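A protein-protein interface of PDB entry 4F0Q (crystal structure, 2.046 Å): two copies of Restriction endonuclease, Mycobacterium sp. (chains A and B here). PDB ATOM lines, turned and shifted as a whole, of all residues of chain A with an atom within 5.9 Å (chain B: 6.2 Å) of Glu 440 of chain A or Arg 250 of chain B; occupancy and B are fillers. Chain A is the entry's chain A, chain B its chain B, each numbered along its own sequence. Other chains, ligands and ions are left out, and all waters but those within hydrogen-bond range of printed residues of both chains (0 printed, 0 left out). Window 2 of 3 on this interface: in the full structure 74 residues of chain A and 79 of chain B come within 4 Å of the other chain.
Of the printed residues of chain B, Arg 306 of chain A touches Gln 251 (3.7 Å). Printed residues of chain B within 4 Å of Tyr 426 of chain A: Arg 250 and Gln 251. Of chain B, only Arg 250 (3.8 Å) and Gln 251 (3.1 Å) come within 4 Å of Glu 440 of chain A. Of the printed residues of chain A, Arg 150 of chain B touches Asn 425. Arg 250 of chain B touches two residues of chain A. Of the printed residues of chain A, Gln 251 of chain B touches Arg 306 (3.7 Å), Asn 425 (3.7 Å), Tyr 426 (3.2 Å) and Glu 440 (3.1 Å). Of the printed residues of chain A, Gly 252 of chain B touches Asn 425. The nearest residue of chain B that does not touch Glu 440 of chain A is Arg 247 of chain B (6.0 Å). The nearest residue of chain A that does not touch Arg 250 of chain B is Asn 425 of chain A (5.2 Å).
Of the 11 printed residues of chain B, 4 touch a printed residue of chain A. Printed residues of chain B that touch a printed residue of chain A: Arg 150, Arg 250, Gln 251 and Gly 252. Hydrophobic or aromatic side chains of chain A that line the printed part of chain B: Tyr 426. Among the printed residues, 8 pairs touch across the chains.
No position is printed for both chains. Of the 8 pairs that touch across the chains among the printed residues, none has its exchanged pair printed and touching as well.
The backbone carbonyl oxygen (O) of Val 249 of chain B is in hydrogen-bond range of the guanidinium group (NE) of Arg 150 of chain B, at 2.9 Å. NE2 of Gln 251 of chain B sits close to NH2 of Arg 250 of chain B, at 3.4 Å. NH1 of Arg 306 of chain A is in hydrogen-bond range of OG of Ser 436 of chain A (2.9 Å). The guanidinium group of Arg 150 of chain B lies within hydrogen-bond range of the backbone carbonyl oxygen of Trp 248 of chain B. The guanidinium group (NH2) of Arg 306 of chain A is in salt-bridge range of the side-chain carboxylate (OE1) of Glu 440 of chain A (3.1 Å). The guanidinium group (NE) of Arg 247 of chain B lies within hydrogen-bond range of the side-chain amide oxygen (OE1) of Gln 251 of chain B (3.1 Å).
The side-chain carboxylate of Glu 440 of chain A lies within salt-bridge range of the guanidinium group of Arg 250 of chain B, at 3.8 Å. The side-chain carboxylate (OE1) of Glu 440 of chain A lies within hydrogen-bond range of the side-chain amide nitrogen (NE2) of Gln 251 of chain B, at 3.1 Å. The guanidinium group of Arg 150 of chain B is in hydrogen-bond range of the backbone carbonyl oxygen of Asn 425 of chain A (3.0 Å). OH of Tyr 426 of chain A lies within hydrogen-bond range of O of Gln 251 of chain B.
Arg 306 of chain A touches Gln 251 of chain B. Asn 425 of chain A touches Gln 251 of chain B. Gly 252 of chain B touches Asn 425 of chain A. Tyr 426 of chain A touches Arg 250 of chain B (CE1 to O, 3.8 Å).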
ATOM      1  N   LEU A 302     -12.158  25.952  21.695  1.00  0.00           N
ATOM      2  CA  LEU A 302     -13.288  25.600  20.834  1.00  0.00           C
ATOM      3  C   LEU A 302     -13.171  26.281  19.471  1.00  0.00           C
ATOM      4  O   LEU A 302     -13.331  25.641  18.415  1.00  0.00           O
ATOM      5  CB  LEU A 302     -14.610  25.983  21.501  1.00  0.00           C
ATOM      6  CG  LEU A 302     -15.883  25.620  20.734  1.00  0.00           C
ATOM      7  CD1 LEU A 302     -15.956  24.119  20.495  1.00  0.00           C
ATOM      8  CD2 LEU A 302     -17.118  26.107  21.473  1.00  0.00           C
ATOM      9  N   ARG A 306     -12.829  24.578  15.712  1.00  0.00           N
ATOM     10  CA  ARG A 306     -13.617  24.922  14.529  1.00  0.00           C
ATOM     11  C   ARG A 306     -12.741  25.406  13.371  1.00  0.00           C
ATOM     12  O   ARG A 306     -12.935  25.009  12.218  1.00  0.00           O
ATOM     13  CB  ARG A 306     -14.678  25.971  14.872  1.00  0.00           C
ATOM     14  CG  ARG A 306     -15.756  25.464  15.816  1.00  0.00           C
ATOM     15  CD  ARG A 306     -16.843  26.501  16.028  1.00  0.00           C
ATOM     16  NE  ARG A 306     -17.898  26.011  16.910  1.00  0.00           N
ATOM     17  CZ  ARG A 306     -18.974  26.714  17.251  1.00  0.00           C
ATOM     18  NH1 ARG A 306     -19.141  27.943  16.783  1.00  0.00           N
ATOM     19  NH2 ARG A 306     -19.882  26.187  18.060  1.00  0.00           N
ATOM     20  N   ASN A 425     -20.935  32.405   7.352  1.00  0.00           N
ATOM     21  CA  ASN A 425     -21.892  31.749   8.241  1.00  0.00           C
ATOM     22  C   ASN A 425     -22.747  32.679   9.101  1.00  0.00           C
ATOM     23  O   ASN A 425     -23.901  32.370   9.394  1.00  0.00           O
ATOM     24  CB  ASN A 425     -21.184  30.727   9.133  1.00  0.00           C
ATOM     25  CG  ASN A 425     -20.554  29.604   8.341  1.00  0.00           C
ATOM     26  OD1 ASN A 425     -21.246  28.711   7.854  1.00  0.00           O
ATOM     27  ND2 ASN A 425     -19.233  29.640   8.209  1.00  0.00           N
ATOM     28  N   TYR A 426     -22.185  33.816   9.502  1.00  0.00           N
ATOM     29  CA  TYR A 426     -22.863  34.691  10.453  1.00  0.00           C
ATOM     30  C   TYR A 426     -23.052  36.116   9.945  1.00  0.00           C
ATOM     31  O   TYR A 426     -23.094  37.061  10.732  1.00  0.00           O
ATOM     32  CB  TYR A 426     -22.115  34.699  11.786  1.00  0.00           C
ATOM     33  CG  TYR A 426     -21.891  33.316  12.349  1.00  0.00           C
ATOM     34  CD1 TYR A 426     -22.957  32.554  12.809  1.00  0.00           C
ATOM     35  CD2 TYR A 426     -20.615  32.770  12.417  1.00  0.00           C
ATOM     36  CE1 TYR A 426     -22.758  31.287  13.322  1.00  0.00           C
ATOM     37  CE2 TYR A 426     -20.408  31.502  12.929  1.00  0.00           C
ATOM     38  CZ  TYR A 426     -21.484  30.766  13.380  1.00  0.00           C
ATOM     39  OH  TYR A 426     -21.285  29.505  13.892  1.00  0.00           O
ATOM     40  N   ALA A 435     -19.198  34.679  20.747  1.00  0.00           N
ATOM     41  CA  ALA A 435     -20.178  34.362  21.779  1.00  0.00           C
ATOM     42  C   ALA A 435     -20.592  32.899  21.709  1.00  0.00           C
ATOM     43  O   ALA A 435     -20.886  32.282  22.732  1.00  0.00           O
ATOM     44  CB  ALA A 435     -21.397  35.265  21.656  1.00  0.00           C
ATOM     45  N   SER A 436     -20.621  32.350  20.498  1.00  0.00           N
ATOM     46  CA  SER A 436     -20.866  30.922  20.330  1.00  0.00           C
ATOM     47  C   SER A 436     -19.788  30.115  21.047  1.00  0.00           C
ATOM     48  O   SER A 436     -20.091  29.179  21.792  1.00  0.00           O
ATOM     49  CB  SER A 436     -20.907  30.550  18.848  1.00  0.00           C
ATOM     50  OG  SER A 436     -21.045  29.151  18.677  1.00  0.00           O
ATOM     51  N   THR A 437     -18.531  30.492  20.829  1.00  0.00           N
ATOM     52  CA  THR A 437     -17.407  29.802  21.457  1.00  0.00           C
ATOM     53  C   THR A 437     -17.429  29.935  22.978  1.00  0.00           C
ATOM     54  O   THR A 437     -17.085  28.994  23.696  1.00  0.00           O
ATOM     55  CB  THR A 437     -16.048  30.304  20.926  1.00  0.00           C
ATOM     56  OG1 THR A 437     -15.895  31.697  21.225  1.00  0.00           O
ATOM     57  CG2 THR A 437     -15.953  30.093  19.420  1.00  0.00           C
ATOM     58  N   VAL A 438     -17.830  31.106  23.467  1.00  0.00           N
ATOM     59  CA  VAL A 438     -17.915  31.334  24.907  1.00  0.00           C
ATOM     60  C   VAL A 438     -19.040  30.515  25.539  1.00  0.00           C
ATOM     61  O   VAL A 438     -18.887  29.965  26.631  1.00  0.00           O
ATOM     62  CB  VAL A 438     -18.115  32.831  25.231  1.00  0.00           C
ATOM     63  CG1 VAL A 438     -18.399  33.034  26.712  1.00  0.00           C
ATOM     64  CG2 VAL A 438     -16.895  33.624  24.815  1.00  0.00           C
ATOM     65  N   ASP A 439     -20.166  30.423  24.839  1.00  0.00           N
ATOM     66  CA  ASP A 439     -21.348  29.763  25.384  1.00  0.00           C
ATOM     67  C   ASP A 439     -21.339  28.244  25.229  1.00  0.00           C
ATOM     68  O   ASP A 439     -22.034  27.541  25.964  1.00  0.00           O
ATOM     69  CB  ASP A 439     -22.619  30.330  24.746  1.00  0.00           C
ATOM     70  CG  ASP A 439     -22.835  31.792  25.072  1.00  0.00           C
ATOM     71  OD1 ASP A 439     -22.478  32.212  26.192  1.00  0.00           O
ATOM     72  OD2 ASP A 439     -23.360  32.523  24.206  1.00  0.00           O
ATOM     73  N   GLU A 440     -20.563  27.732  24.280  1.00  0.00           N
ATOM     74  CA  GLU A 440     -20.655  26.313  23.949  1.00  0.00           C
ATOM     75  C   GLU A 440     -19.394  25.483  24.205  1.00  0.00           C
ATOM     76  O   GLU A 440     -19.340  24.315  23.821  1.00  0.00           O
ATOM     77  CB  GLU A 440     -21.105  26.141  22.494  1.00  0.00           C
ATOM     78  CG  GLU A 440     -22.422  26.828  22.169  1.00  0.00           C
ATOM     79  CD  GLU A 440     -22.846  26.627  20.727  1.00  0.00           C
ATOM     80  OE1 GLU A 440     -22.199  25.824  20.024  1.00  0.00           O
ATOM     81  OE2 GLU A 440     -23.825  27.273  20.298  1.00  0.00           O
ATOM     82  N   TYR A 441     -18.389  26.061  24.854  1.00  0.00           N
ATOM     83  CA  TYR A 441     -17.138  25.333  25.064  1.00  0.00           C
ATOM     84  C   TYR A 441     -17.235  24.276  26.165  1.00  0.00           C
ATOM     85  O   TYR A 441     -16.564  23.246  26.106  1.00  0.00           O
ATOM     86  CB  TYR A 441     -15.958  26.285  25.310  1.00  0.00           C
ATOM     87  CG  TYR A 441     -15.883  26.885  26.698  1.00  0.00           C
ATOM     88  CD1 TYR A 441     -15.215  26.230  27.727  1.00  0.00           C
ATOM     89  CD2 TYR A 441     -16.457  28.120  26.973  1.00  0.00           C
ATOM     90  CE1 TYR A 441     -15.138  26.779  28.994  1.00  0.00           C
ATOM     91  CE2 TYR A 441     -16.384  28.677  28.238  1.00  0.00           C
ATOM     92  CZ  TYR A 441     -15.722  28.003  29.243  1.00  0.00           C
ATOM     93  OH  TYR A 441     -15.645  28.550  30.503  1.00  0.00           O
ATOM     94  N   GLY A 442     -18.072  24.534  27.165  1.00  0.00           N
ATOM     95  CA  GLY A 442     -18.244  23.605  28.267  1.00  0.00           C
ATOM     96  C   GLY A 442     -18.913  22.308  27.852  1.00  0.00           C
ATOM     97  O   GLY A 442     -18.561  21.233  28.339  1.00  0.00           O
ATOM     98  N   ALA A 443     -19.879  22.408  26.944  1.00  0.00           N
ATOM     99  CA  ALA A 443     -20.629  21.242  26.486  1.00  0.00           C
ATOM    100  C   ALA A 443     -19.894  20.484  25.384  1.00  0.00           C
ATOM    101  O   ALA A 443     -20.370  19.455  24.903  1.00  0.00           O
ATOM    102  CB  ALA A 443     -22.015  21.656  26.011  1.00  0.00           C
ATOM    103  N   ALA A 444     -18.733  20.995  24.987  1.00  0.00           N
ATOM    104  CA  ALA A 444     -17.929  20.357  23.952  1.00  0.00           C
ATOM    105  C   ALA A 444     -16.814  19.526  24.574  1.00  0.00           C
ATOM    106  O   ALA A 444     -15.884  19.103  23.890  1.00  0.00           O
ATOM    107  CB  ALA A 444     -17.348  21.405  23.015  1.00  0.00           C
ATOM    108  N   ARG B 147     -28.490  32.708   9.212  1.00  0.00           N
ATOM    109  CA  ARG B 147     -29.464  31.744   9.703  1.00  0.00           C
ATOM    110  C   ARG B 147     -30.775  31.887   8.939  1.00  0.00           C
ATOM    111  O   ARG B 147     -31.466  30.904   8.685  1.00  0.00           O
ATOM    112  CB  ARG B 147     -29.702  31.927  11.204  1.00  0.00           C
ATOM    113  CG  ARG B 147     -30.751  30.983  11.761  1.00  0.00           C
ATOM    114  CD  ARG B 147     -30.895  31.093  13.264  1.00  0.00           C
ATOM    115  NE  ARG B 147     -31.808  30.078  13.778  1.00  0.00           N
ATOM    116  CZ  ARG B 147     -33.124  30.236  13.875  1.00  0.00           C
ATOM    117  NH1 ARG B 147     -33.686  31.375  13.498  1.00  0.00           N
ATOM    118  NH2 ARG B 147     -33.878  29.255  14.352  1.00  0.00           N
ATOM    119  N   ARG B 150     -30.486  29.964   5.714  1.00  0.00           N
ATOM    120  CA  ARG B 150     -30.476  28.528   5.978  1.00  0.00           C
ATOM    121  C   ARG B 150     -31.839  28.029   6.447  1.00  0.00           C
ATOM    122  O   ARG B 150     -32.128  26.835   6.379  1.00  0.00           O
ATOM    123  CB  ARG B 150     -29.392  28.171   6.997  1.00  0.00           C
ATOM    124  CG  ARG B 150     -27.976  28.386   6.488  1.00  0.00           C
ATOM    125  CD  ARG B 150     -26.943  27.849   7.465  1.00  0.00           C
ATOM    126  NE  ARG B 150     -26.969  28.553   8.743  1.00  0.00           N
ATOM    127  CZ  ARG B 150     -26.236  29.627   9.016  1.00  0.00           C
ATOM    128  NH1 ARG B 150     -25.417  30.123   8.100  1.00  0.00           N
ATOM    129  NH2 ARG B 150     -26.320  30.205  10.206  1.00  0.00           N
ATOM    130  N   GLU B 243     -32.776  17.898  15.855  1.00  0.00           N
ATOM    131  CA  GLU B 243     -31.951  18.859  16.581  1.00  0.00           C
ATOM    132  C   GLU B 243     -30.667  19.191  15.830  1.00  0.00           C
ATOM    133  O   GLU B 243     -30.156  20.306  15.922  1.00  0.00           O
ATOM    134  CB  GLU B 243     -31.624  18.341  17.983  1.00  0.00           C
ATOM    135  CG  GLU B 243     -32.836  18.207  18.894  1.00  0.00           C
ATOM    136  CD  GLU B 243     -33.508  19.540  19.175  1.00  0.00           C
ATOM    137  OE1 GLU B 243     -32.807  20.573  19.181  1.00  0.00           O
ATOM    138  OE2 GLU B 243     -34.739  19.553  19.389  1.00  0.00           O
ATOM    139  N   TRP B 245     -30.427  19.443  12.656  1.00  0.00           N
ATOM    140  CA  TRP B 245     -30.794  20.382  11.606  1.00  0.00           C
ATOM    141  C   TRP B 245     -30.962  21.788  12.166  1.00  0.00           C
ATOM    142  O   TRP B 245     -30.609  22.766  11.512  1.00  0.00           O
ATOM    143  CB  TRP B 245     -32.071  19.945  10.890  1.00  0.00           C
ATOM    144  CG  TRP B 245     -32.261  20.647   9.584  1.00  0.00           C
ATOM    145  CD1 TRP B 245     -32.806  21.883   9.388  1.00  0.00           C
ATOM    146  CD2 TRP B 245     -31.890  20.163   8.289  1.00  0.00           C
ATOM    147  NE1 TRP B 245     -32.801  22.195   8.050  1.00  0.00           N
ATOM    148  CE2 TRP B 245     -32.244  21.154   7.354  1.00  0.00           C
ATOM    149  CE3 TRP B 245     -31.298  18.982   7.829  1.00  0.00           C
ATOM    150  CZ2 TRP B 245     -32.026  21.002   5.987  1.00  0.00           C
ATOM    151  CZ3 TRP B 245     -31.081  18.834   6.473  1.00  0.00           C
ATOM    152  CH2 TRP B 245     -31.442  19.839   5.567  1.00  0.00           C
ATOM    153  N   ILE B 246     -31.509  21.882  13.374  1.00  0.00           N
ATOM    154  CA  ILE B 246     -31.655  23.163  14.053  1.00  0.00           C
ATOM    155  C   ILE B 246     -30.271  23.735  14.346  1.00  0.00           C
ATOM    156  O   ILE B 246     -30.024  24.939  14.192  1.00  0.00           O
ATOM    157  CB  ILE B 246     -32.446  23.007  15.366  1.00  0.00           C
ATOM    158  CG1 ILE B 246     -33.837  22.438  15.078  1.00  0.00           C
ATOM    159  CG2 ILE B 246     -32.554  24.336  16.094  1.00  0.00           C
ATOM    160  CD1 ILE B 246     -34.669  22.191  16.315  1.00  0.00           C
ATOM    161  N   ARG B 247     -29.369  22.848  14.755  1.00  0.00           N
ATOM    162  CA  ARG B 247     -27.983  23.214  15.008  1.00  0.00           C
ATOM    163  C   ARG B 247     -27.311  23.715  13.736  1.00  0.00           C
ATOM    164  O   ARG B 247     -26.528  24.658  13.779  1.00  0.00           O
ATOM    165  CB  ARG B 247     -27.203  22.026  15.575  1.00  0.00           C
ATOM    166  CG  ARG B 247     -25.753  22.350  15.883  1.00  0.00           C
ATOM    167  CD  ARG B 247     -24.934  21.101  16.148  1.00  0.00           C
ATOM    168  NE  ARG B 247     -23.504  21.390  16.129  1.00  0.00           N
ATOM    169  CZ  ARG B 247     -22.553  20.467  16.220  1.00  0.00           C
ATOM    170  NH1 ARG B 247     -22.879  19.186  16.339  1.00  0.00           N
ATOM    171  NH2 ARG B 247     -21.276  20.824  16.193  1.00  0.00           N
ATOM    172  N   TRP B 248     -27.612  23.082  12.605  1.00  0.00           N
ATOM    173  CA  TRP B 248     -27.050  23.524  11.333  1.00  0.00           C
ATOM    174  C   TRP B 248     -27.627  24.865  10.891  1.00  0.00           C
ATOM    175  O   TRP B 248     -26.925  25.688  10.312  1.00  0.00           O
ATOM    176  CB  TRP B 248     -27.261  22.488  10.229  1.00  0.00           C
ATOM    177  CG  TRP B 248     -26.963  23.053   8.872  1.00  0.00           C
ATOM    178  CD1 TRP B 248     -25.732  23.214   8.303  1.00  0.00           C
ATOM    179  CD2 TRP B 248     -27.911  23.559   7.925  1.00  0.00           C
ATOM    180  NE1 TRP B 248     -25.856  23.779   7.059  1.00  0.00           N
ATOM    181  CE2 TRP B 248     -27.183  24.001   6.803  1.00  0.00           C
ATOM    182  CE3 TRP B 248     -29.304  23.677   7.916  1.00  0.00           C
ATOM    183  CZ2 TRP B 248     -27.803  24.551   5.681  1.00  0.00           C
ATOM    184  CZ3 TRP B 248     -29.916  24.224   6.802  1.00  0.00           C
ATOM    185  CH2 TRP B 248     -29.167  24.653   5.700  1.00  0.00           C
ATOM    186  N   VAL B 249     -28.912  25.073  11.150  1.00  0.00           N
ATOM    187  CA  VAL B 249     -29.552  26.337  10.815  1.00  0.00           C
ATOM    188  C   VAL B 249     -28.913  27.457  11.630  1.00  0.00           C
ATOM    189  O   VAL B 249     -28.696  28.560  11.124  1.00  0.00           O
ATOM    190  CB  VAL B 249     -31.078  26.284  11.053  1.00  0.00           C
ATOM    191  CG1 VAL B 249     -31.692  27.662  10.921  1.00  0.00           C
ATOM    192  CG2 VAL B 249     -31.731  25.322  10.074  1.00  0.00           C
ATOM    193  N   ARG B 250     -28.578  27.156  12.882  1.00  0.00           N
ATOM    194  CA  ARG B 250     -27.927  28.137  13.749  1.00  0.00           C
ATOM    195  C   ARG B 250     -26.463  28.412  13.381  1.00  0.00           C
ATOM    196  O   ARG B 250     -26.083  29.557  13.140  1.00  0.00           O
ATOM    197  CB  ARG B 250     -28.016  27.702  15.214  1.00  0.00           C
ATOM    198  CG  ARG B 250     -27.361  28.674  16.186  1.00  0.00           C
ATOM    199  CD  ARG B 250     -27.498  28.218  17.635  1.00  0.00           C
ATOM    200  NE  ARG B 250     -26.761  26.985  17.909  1.00  0.00           N
ATOM    201  CZ  ARG B 250     -27.326  25.791  18.061  1.00  0.00           C
ATOM    202  NH1 ARG B 250     -28.643  25.659  17.973  1.00  0.00           N
ATOM    203  NH2 ARG B 250     -26.572  24.728  18.306  1.00  0.00           N
ATOM    204  N   GLN B 251     -25.654  27.358  13.339  1.00  0.00           N
ATOM    205  CA  GLN B 251     -24.204  27.481  13.190  1.00  0.00           C
ATOM    206  C   GLN B 251     -23.736  27.566  11.738  1.00  0.00           C
ATOM    207  O   GLN B 251     -22.858  28.363  11.405  1.00  0.00           O
ATOM    208  CB  GLN B 251     -23.507  26.310  13.886  1.00  0.00           C
ATOM    209  CG  GLN B 251     -23.816  26.196  15.369  1.00  0.00           C
ATOM    210  CD  GLN B 251     -23.135  25.006  16.014  1.00  0.00           C
ATOM    211  OE1 GLN B 251     -22.470  24.219  15.340  1.00  0.00           O
ATOM    212  NE2 GLN B 251     -23.299  24.866  17.325  1.00  0.00           N
ATOM    213  N   GLY B 252     -24.310  26.728  10.883  1.00  0.00           N
ATOM    214  CA  GLY B 252     -23.983  26.735   9.470  1.00  0.00           C
ATOM    215  C   GLY B 252     -22.972  25.672   9.088  1.00  0.00           C
ATOM    216  O   GLY B 252     -23.123  24.501   9.437  1.00  0.00           O
